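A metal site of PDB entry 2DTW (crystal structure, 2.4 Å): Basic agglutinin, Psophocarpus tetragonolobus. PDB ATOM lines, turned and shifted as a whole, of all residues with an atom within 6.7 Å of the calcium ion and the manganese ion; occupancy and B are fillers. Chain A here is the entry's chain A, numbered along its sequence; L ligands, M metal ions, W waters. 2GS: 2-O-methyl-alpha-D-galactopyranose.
O3 of the ligand lies within hydrogen-bond range of ND2 of Asn 128, 3.2 Å away. N of Gly 105 sits at hydrogen-bond distance from O3 of the ligand (3.0 Å). O3 of the ligand sits at hydrogen-bond distance from OD2 of Asp 87 (2.7 Å).
OD1 of Asp 131 sits close to NE1 of Trp 130, 3.3 Å away. The guanidinium group (NE) of Arg 127 lies within hydrogen-bond range of the backbone carbonyl oxygen (O) of Asp 131, 3.0 Å away. The side-chain carboxylate (OE1) of Glu 122 lies close to the side-chain carboxylate (OD2) of Asp 140, at 2.7 Å. O of Gly 138 lies within hydrogen-bond range of N of Glu 122 (2.9 Å). N of Phe 126 lies within hydrogen-bond range of O of Asp 87 (3.5 Å).
OD2 of Asp 131 binds the calcium ion (2.3 Å). Water W4 is bound to the calcium ion, at 2.3 Å. The calcium ion is bound by water W2 (2.4 Å). The calcium ion is bound by O of Phe 126 (2.4 Å). The side-chain carboxylate (OD2) of Asp 124 binds the calcium ion, at 2.5 Å. OD1 of Asp 124 is bound to the calcium ion (2.5 Å). The calcium ion is bound by OD1 of Asn 128, 2.9 Å away. The calcium ion has seven donor atoms within binding distance.
Within 4 Å of the manganese ion: Glu 122, Asp 124, Asp 131 and His 136.
Water W2 lies within hydrogen-bond range of the backbone carbonyl oxygen (O) of Gly 105 (2.8 Å) and the indole nitrogen (NE1) of Trp 130 (3.3 Å). Water W3 lies within hydrogen-bond range of OE1 of Glu 122 (2.7 Å), O of Val 144 (2.8 Å) and NE1 of Trp 130 (3.3 Å).
The manganese ion is bound by the side-chain carboxylate (OD1) of Asp 131 (2.2 Å), the side-chain carboxylate (OE2) of Glu 122 (2.3 Å), water W3 (2.3 Å), water W1 (2.3 Å), the side-chain carboxylate (OD2) of Asp 124 (2.3 Å) and a ring nitrogen (NE2) of His 136 (2.3 Å).
Within 4 Å of the calcium ion: Asp 124, Phe 126, Asn 128 and Asp 131.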
ATOM      1  N   ASP A  87       1.566 -19.313   2.962  1.00  0.00           N
ATOM      2  CA  ASP A  87       2.145 -19.351   4.307  1.00  0.00           C
ATOM      3  C   ASP A  87       2.017 -17.996   5.019  1.00  0.00           C
ATOM      4  O   ASP A  87       1.989 -17.938   6.240  1.00  0.00           O
ATOM      5  CB  ASP A  87       3.630 -19.730   4.246  1.00  0.00           C
ATOM      6  CG  ASP A  87       3.836 -21.221   4.255  1.00  0.00           C
ATOM      7  OD1 ASP A  87       3.845 -21.829   3.155  1.00  0.00           O
ATOM      8  OD2 ASP A  87       3.966 -21.785   5.367  1.00  0.00           O
ATOM      9  N   GLY A 104       8.083 -21.495   2.063  1.00  0.00           N
ATOM     10  CA  GLY A 104       7.256 -22.024   3.129  1.00  0.00           C
ATOM     11  C   GLY A 104       7.209 -21.140   4.358  1.00  0.00           C
ATOM     12  O   GLY A 104       7.106 -19.907   4.251  1.00  0.00           O
ATOM     13  N   GLY A 105       7.290 -21.753   5.535  1.00  0.00           N
ATOM     14  CA  GLY A 105       7.255 -20.998   6.782  1.00  0.00           C
ATOM     15  C   GLY A 105       8.376 -20.000   6.993  1.00  0.00           C
ATOM     16  O   GLY A 105       8.342 -19.250   7.962  1.00  0.00           O
ATOM     17  N   TYR A 106       9.359 -19.985   6.102  1.00  0.00           N
ATOM     18  CA  TYR A 106      10.459 -19.042   6.219  1.00  0.00           C
ATOM     19  C   TYR A 106      10.204 -17.755   5.412  1.00  0.00           C
ATOM     20  O   TYR A 106      11.030 -16.836   5.399  1.00  0.00           O
ATOM     21  CB  TYR A 106      11.761 -19.708   5.780  1.00  0.00           C
ATOM     22  CG  TYR A 106      12.157 -20.835   6.704  1.00  0.00           C
ATOM     23  CD1 TYR A 106      12.522 -20.587   8.024  1.00  0.00           C
ATOM     24  CD2 TYR A 106      12.115 -22.167   6.279  1.00  0.00           C
ATOM     25  CE1 TYR A 106      12.830 -21.626   8.901  1.00  0.00           C
ATOM     26  CE2 TYR A 106      12.415 -23.208   7.144  1.00  0.00           C
ATOM     27  CZ  TYR A 106      12.777 -22.933   8.452  1.00  0.00           C
ATOM     28  OH  TYR A 106      13.063 -23.972   9.317  1.00  0.00           O
ATOM     29  N   PHE A 107       9.049 -17.727   4.747  1.00  0.00           N
ATOM     30  CA  PHE A 107       8.608 -16.559   3.994  1.00  0.00           C
ATOM     31  C   PHE A 107       9.540 -16.042   2.907  1.00  0.00           C
ATOM     32  O   PHE A 107       9.242 -15.033   2.275  1.00  0.00           O
ATOM     33  CB  PHE A 107       8.332 -15.409   4.966  1.00  0.00           C
ATOM     34  CG  PHE A 107       7.363 -15.760   6.067  1.00  0.00           C
ATOM     35  CD1 PHE A 107       6.043 -16.071   5.783  1.00  0.00           C
ATOM     36  CD2 PHE A 107       7.778 -15.740   7.393  1.00  0.00           C
ATOM     37  CE1 PHE A 107       5.131 -16.364   6.813  1.00  0.00           C
ATOM     38  CE2 PHE A 107       6.887 -16.033   8.434  1.00  0.00           C
ATOM     39  CZ  PHE A 107       5.561 -16.336   8.152  1.00  0.00           C
ATOM     40  N   GLU A 122       5.483 -10.213  10.584  1.00  0.00           N
ATOM     41  CA  GLU A 122       4.832 -11.242   9.800  1.00  0.00           C
ATOM     42  C   GLU A 122       3.333 -11.312  10.019  1.00  0.00           C
ATOM     43  O   GLU A 122       2.812 -10.982  11.078  1.00  0.00           O
ATOM     44  CB  GLU A 122       5.414 -12.620  10.145  1.00  0.00           C
ATOM     45  CG  GLU A 122       5.193 -13.006  11.590  1.00  0.00           C
ATOM     46  CD  GLU A 122       5.502 -14.464  11.892  1.00  0.00           C
ATOM     47  OE1 GLU A 122       6.607 -14.934  11.545  1.00  0.00           O
ATOM     48  OE2 GLU A 122       4.633 -15.122  12.495  1.00  0.00           O
ATOM     49  N   ASP A 124       1.378 -14.270   9.542  1.00  0.00           N
ATOM     50  CA  ASP A 124       1.463 -15.711   9.414  1.00  0.00           C
ATOM     51  C   ASP A 124       0.117 -16.399   9.281  1.00  0.00           C
ATOM     52  O   ASP A 124      -0.722 -16.291  10.160  1.00  0.00           O
ATOM     53  CB  ASP A 124       2.179 -16.255  10.648  1.00  0.00           C
ATOM     54  CG  ASP A 124       2.891 -17.541  10.320  1.00  0.00           C
ATOM     55  OD1 ASP A 124       2.925 -17.950   9.122  1.00  0.00           O
ATOM     56  OD2 ASP A 124       3.415 -18.153  11.264  1.00  0.00           O
ATOM     57  N   THR A 125      -0.064 -17.158   8.202  1.00  0.00           N
ATOM     58  CA  THR A 125      -1.324 -17.850   7.966  1.00  0.00           C
ATOM     59  C   THR A 125      -1.265 -19.370   8.148  1.00  0.00           C
ATOM     60  O   THR A 125      -2.302 -20.031   8.189  1.00  0.00           O
ATOM     61  CB  THR A 125      -1.821 -17.553   6.569  1.00  0.00           C
ATOM     62  OG1 THR A 125      -0.766 -17.772   5.629  1.00  0.00           O
ATOM     63  CG2 THR A 125      -2.309 -16.098   6.480  1.00  0.00           C
ATOM     64  N   PHE A 126      -0.051 -19.915   8.237  1.00  0.00           N
ATOM     65  CA  PHE A 126       0.111 -21.357   8.399  1.00  0.00           C
ATOM     66  C   PHE A 126       0.833 -21.678   9.703  1.00  0.00           C
ATOM     67  O   PHE A 126       1.881 -21.091  10.008  1.00  0.00           O
ATOM     68  CB  PHE A 126       0.899 -21.954   7.236  1.00  0.00           C
ATOM     69  CG  PHE A 126       1.165 -23.416   7.397  1.00  0.00           C
ATOM     70  CD1 PHE A 126       0.202 -24.352   7.066  1.00  0.00           C
ATOM     71  CD2 PHE A 126       2.369 -23.852   7.960  1.00  0.00           C
ATOM     72  CE1 PHE A 126       0.415 -25.720   7.300  1.00  0.00           C
ATOM     73  CE2 PHE A 126       2.591 -25.205   8.211  1.00  0.00           C
ATOM     74  CZ  PHE A 126       1.615 -26.136   7.871  1.00  0.00           C
ATOM     75  N   ARG A 127       0.304 -22.635  10.451  1.00  0.00           N
ATOM     76  CA  ARG A 127       0.915 -22.985  11.728  1.00  0.00           C
ATOM     77  C   ARG A 127       2.028 -24.013  11.639  1.00  0.00           C
ATOM     78  O   ARG A 127       1.780 -25.207  11.550  1.00  0.00           O
ATOM     79  CB  ARG A 127      -0.148 -23.471  12.712  1.00  0.00           C
ATOM     80  CG  ARG A 127       0.410 -23.674  14.103  1.00  0.00           C
ATOM     81  CD  ARG A 127      -0.652 -24.023  15.126  1.00  0.00           C
ATOM     82  NE  ARG A 127      -0.125 -23.910  16.491  1.00  0.00           N
ATOM     83  CZ  ARG A 127      -0.825 -24.156  17.590  1.00  0.00           C
ATOM     84  NH1 ARG A 127      -2.086 -24.560  17.499  1.00  0.00           N
ATOM     85  NH2 ARG A 127      -0.262 -23.986  18.785  1.00  0.00           N
ATOM     86  N   ASN A 128       3.271 -23.530  11.683  1.00  0.00           N
ATOM     87  CA  ASN A 128       4.436 -24.417  11.669  1.00  0.00           C
ATOM     88  C   ASN A 128       4.617 -24.956  13.090  1.00  0.00           C
ATOM     89  O   ASN A 128       3.899 -24.558  14.005  1.00  0.00           O
ATOM     90  CB  ASN A 128       5.688 -23.646  11.253  1.00  0.00           C
ATOM     91  CG  ASN A 128       5.860 -23.482   9.746  1.00  0.00           C
ATOM     92  OD1 ASN A 128       5.611 -22.416   9.190  1.00  0.00           O
ATOM     93  ND2 ASN A 128       6.293 -24.559   9.085  1.00  0.00           N
ATOM     94  N   TRP A 130       6.799 -24.272  15.221  1.00  0.00           N
ATOM     95  CA  TRP A 130       7.227 -23.192  16.107  1.00  0.00           C
ATOM     96  C   TRP A 130       6.180 -22.096  16.277  1.00  0.00           C
ATOM     97  O   TRP A 130       6.432 -21.121  16.989  1.00  0.00           O
ATOM     98  CB  TRP A 130       8.505 -22.572  15.554  1.00  0.00           C
ATOM     99  CG  TRP A 130       8.306 -22.003  14.163  1.00  0.00           C
ATOM    100  CD1 TRP A 130       7.630 -20.865  13.824  1.00  0.00           C
ATOM    101  CD2 TRP A 130       8.762 -22.572  12.930  1.00  0.00           C
ATOM    102  NE1 TRP A 130       7.631 -20.688  12.462  1.00  0.00           N
ATOM    103  CE2 TRP A 130       8.325 -21.724  11.892  1.00  0.00           C
ATOM    104  CE3 TRP A 130       9.505 -23.723  12.597  1.00  0.00           C
ATOM    105  CZ2 TRP A 130       8.593 -21.983  10.537  1.00  0.00           C
ATOM    106  CZ3 TRP A 130       9.772 -23.986  11.252  1.00  0.00           C
ATOM    107  CH2 TRP A 130       9.323 -23.117  10.243  1.00  0.00           C
ATOM    108  N   ASP A 131       5.018 -22.243  15.634  1.00  0.00           N
ATOM    109  CA  ASP A 131       3.960 -21.235  15.676  1.00  0.00           C
ATOM    110  C   ASP A 131       2.826 -21.429  16.655  1.00  0.00           C
ATOM    111  O   ASP A 131       2.477 -22.554  17.011  1.00  0.00           O
ATOM    112  CB  ASP A 131       3.253 -21.087  14.321  1.00  0.00           C
ATOM    113  CG  ASP A 131       4.029 -20.397  13.246  1.00  0.00           C
ATOM    114  OD1 ASP A 131       4.772 -19.453  13.568  1.00  0.00           O
ATOM    115  OD2 ASP A 131       3.858 -20.794  12.064  1.00  0.00           O
ATOM    116  N   PRO A 132       2.220 -20.323  17.105  1.00  0.00           N
ATOM    117  CA  PRO A 132       1.089 -20.376  18.029  1.00  0.00           C
ATOM    118  C   PRO A 132      -0.098 -20.397  17.047  1.00  0.00           C
ATOM    119  O   PRO A 132       0.115 -20.522  15.843  1.00  0.00           O
ATOM    120  CB  PRO A 132       1.192 -19.054  18.773  1.00  0.00           C
ATOM    121  CG  PRO A 132       1.719 -18.135  17.714  1.00  0.00           C
ATOM    122  CD  PRO A 132       2.815 -18.979  17.085  1.00  0.00           C
ATOM    123  N   ILE A 134      -2.961 -19.649  14.395  1.00  0.00           N
ATOM    124  CA  ILE A 134      -2.936 -18.758  13.248  1.00  0.00           C
ATOM    125  C   ILE A 134      -4.374 -18.368  12.890  1.00  0.00           C
ATOM    126  O   ILE A 134      -5.319 -19.069  13.219  1.00  0.00           O
ATOM    127  CB  ILE A 134      -2.203 -19.395  12.026  1.00  0.00           C
ATOM    128  CG1 ILE A 134      -2.811 -20.754  11.679  1.00  0.00           C
ATOM    129  CG2 ILE A 134      -0.714 -19.504  12.306  1.00  0.00           C
ATOM    130  CD1 ILE A 134      -4.151 -20.676  10.916  1.00  0.00           C
ATOM    131  N   HIS A 136      -1.749 -14.969  12.846  1.00  0.00           N
ATOM    132  CA  HIS A 136      -1.215 -14.119  13.889  1.00  0.00           C
ATOM    133  C   HIS A 136      -0.206 -13.135  13.346  1.00  0.00           C
ATOM    134  O   HIS A 136       0.413 -13.366  12.316  1.00  0.00           O
ATOM    135  CB  HIS A 136      -0.569 -14.943  15.020  1.00  0.00           C
ATOM    136  CG  HIS A 136       0.549 -15.835  14.597  1.00  0.00           C
ATOM    137  ND1 HIS A 136       0.365 -17.153  14.265  1.00  0.00           N
ATOM    138  CD2 HIS A 136       1.888 -15.611  14.490  1.00  0.00           C
ATOM    139  CE1 HIS A 136       1.530 -17.712  13.975  1.00  0.00           C
ATOM    140  NE2 HIS A 136       2.463 -16.792  14.107  1.00  0.00           N
ATOM    141  N   ILE A 137      -0.084 -12.007  14.032  1.00  0.00           N
ATOM    142  CA  ILE A 137       0.892 -11.000  13.665  1.00  0.00           C
ATOM    143  C   ILE A 137       2.077 -11.338  14.550  1.00  0.00           C
ATOM    144  O   ILE A 137       1.891 -11.750  15.701  1.00  0.00           O
ATOM    145  CB  ILE A 137       0.438  -9.592  14.029  1.00  0.00           C
ATOM    146  CG1 ILE A 137      -0.909  -9.279  13.393  1.00  0.00           C
ATOM    147  CG2 ILE A 137       1.469  -8.599  13.554  1.00  0.00           C
ATOM    148  CD1 ILE A 137      -1.424  -7.901  13.733  1.00  0.00           C
ATOM    149  N   GLY A 138       3.274 -11.195  14.024  1.00  0.00           N
ATOM    150  CA  GLY A 138       4.435 -11.503  14.833  1.00  0.00           C
ATOM    151  C   GLY A 138       5.586 -10.576  14.542  1.00  0.00           C
ATOM    152  O   GLY A 138       5.714 -10.053  13.439  1.00  0.00           O
ATOM    153  N   ASP A 140       9.520 -10.465  14.291  1.00  0.00           N
ATOM    154  CA  ASP A 140      10.648 -11.367  14.142  1.00  0.00           C
ATOM    155  C   ASP A 140      11.984 -10.660  14.101  1.00  0.00           C
ATOM    156  O   ASP A 140      12.159  -9.685  13.384  1.00  0.00           O
ATOM    157  CB  ASP A 140      10.478 -12.221  12.882  1.00  0.00           C
ATOM    158  CG  ASP A 140       9.099 -12.834  12.763  1.00  0.00           C
ATOM    159  OD1 ASP A 140       8.366 -12.891  13.769  1.00  0.00           O
ATOM    160  OD2 ASP A 140       8.750 -13.280  11.650  1.00  0.00           O
ATOM    161  N   VAL A 144      12.346 -16.697  12.565  1.00  0.00           N
ATOM    162  CA  VAL A 144      10.912 -16.725  12.312  1.00  0.00           C
ATOM    163  C   VAL A 144      10.164 -17.118  13.580  1.00  0.00           C
ATOM    164  O   VAL A 144       8.933 -17.220  13.588  1.00  0.00           O
ATOM    165  CB  VAL A 144      10.581 -17.717  11.154  1.00  0.00           C
ATOM    166  CG1 VAL A 144      11.109 -17.199   9.845  1.00  0.00           C
ATOM    167  CG2 VAL A 144      11.231 -19.063  11.449  1.00  0.00           C
ATOM    168  N   ILE A 145      10.904 -17.365  14.656  1.00  0.00           N
ATOM    169  CA  ILE A 145      10.292 -17.701  15.930  1.00  0.00           C
ATOM    170  C   ILE A 145      10.112 -16.360  16.635  1.00  0.00           C
ATOM    171  O   ILE A 145      11.010 -15.872  17.322  1.00  0.00           O
ATOM    172  CB  ILE A 145      11.207 -18.606  16.758  1.00  0.00           C
ATOM    173  CG1 ILE A 145      11.403 -19.936  16.016  1.00  0.00           C
ATOM    174  CG2 ILE A 145      10.613 -18.854  18.138  1.00  0.00           C
ATOM    175  CD1 ILE A 145      12.403 -20.857  16.693  1.00  0.00           C
ATOM    176  N   SER A 146       8.948 -15.763  16.428  1.00  0.00           N
ATOM    177  CA  SER A 146       8.596 -14.443  16.957  1.00  0.00           C
ATOM    178  C   SER A 146       8.889 -14.198  18.431  1.00  0.00           C
ATOM    179  O   SER A 146       8.751 -15.097  19.262  1.00  0.00           O
ATOM    180  CB  SER A 146       7.115 -14.163  16.706  1.00  0.00           C
ATOM    181  OG  SER A 146       6.795 -14.279  15.341  1.00  0.00           O
ATOM    182  N   THR A 149       3.709 -12.185  19.741  1.00  0.00           N
ATOM    183  CA  THR A 149       2.683 -12.626  18.820  1.00  0.00           C
ATOM    184  C   THR A 149       1.283 -12.233  19.273  1.00  0.00           C
ATOM    185  O   THR A 149       1.009 -12.147  20.480  1.00  0.00           O
ATOM    186  CB  THR A 149       2.791 -14.170  18.698  1.00  0.00           C
ATOM    187  OG1 THR A 149       3.491 -14.504  17.486  1.00  0.00           O
ATOM    188  CG2 THR A 149       1.447 -14.836  18.753  1.00  0.00           C
HETATM  189  C1  2GS L   1       5.386 -27.578   4.865  1.00  0.00           C
HETATM  190  C2  2GS L   1       5.969 -26.142   5.238  1.00  0.00           C
HETATM  191  C3  2GS L   1       4.811 -25.222   5.807  1.00  0.00           C
HETATM  192  C4  2GS L   1       3.653 -25.128   4.751  1.00  0.00           C
HETATM  193  C5  2GS L   1       3.127 -26.565   4.444  1.00  0.00           C
HETATM  194  C6  2GS L   1       2.033 -26.533   3.411  1.00  0.00           C
HETATM  195  C7  2GS L   1       8.173 -25.331   6.224  1.00  0.00           C
HETATM  196  O1  2GS L   1       4.981 -28.312   6.039  1.00  0.00           O
HETATM  197  O2  2GS L   1       7.073 -26.269   6.173  1.00  0.00           O
HETATM  198  O3  2GS L   1       5.324 -23.948   6.129  1.00  0.00           O
HETATM  199  O4  2GS L   1       4.106 -24.471   3.563  1.00  0.00           O
HETATM  200  O5  2GS L   1       4.229 -27.414   3.930  1.00  0.00           O
HETATM  201  O6  2GS L   1       1.550 -27.848   3.129  1.00  0.00           O
HETATM  202 CA    CA M   1       4.073 -20.090   9.850  1.00  0.00          CA
HETATM  203 MN    MN M   2       4.494 -17.299  13.092  1.00  0.00          MN
HETATM  204  O   HOH W   1       5.463 -16.519  14.993  1.00  0.00           O
HETATM  205  O   HOH W   2       6.287 -19.129   9.880  1.00  0.00           O
HETATM  206  O   HOH W   3       6.525 -17.569  12.130  1.00  0.00           O
HETATM  207  O   HOH W   4       3.954 -20.062   7.504  1.00  0.00           O
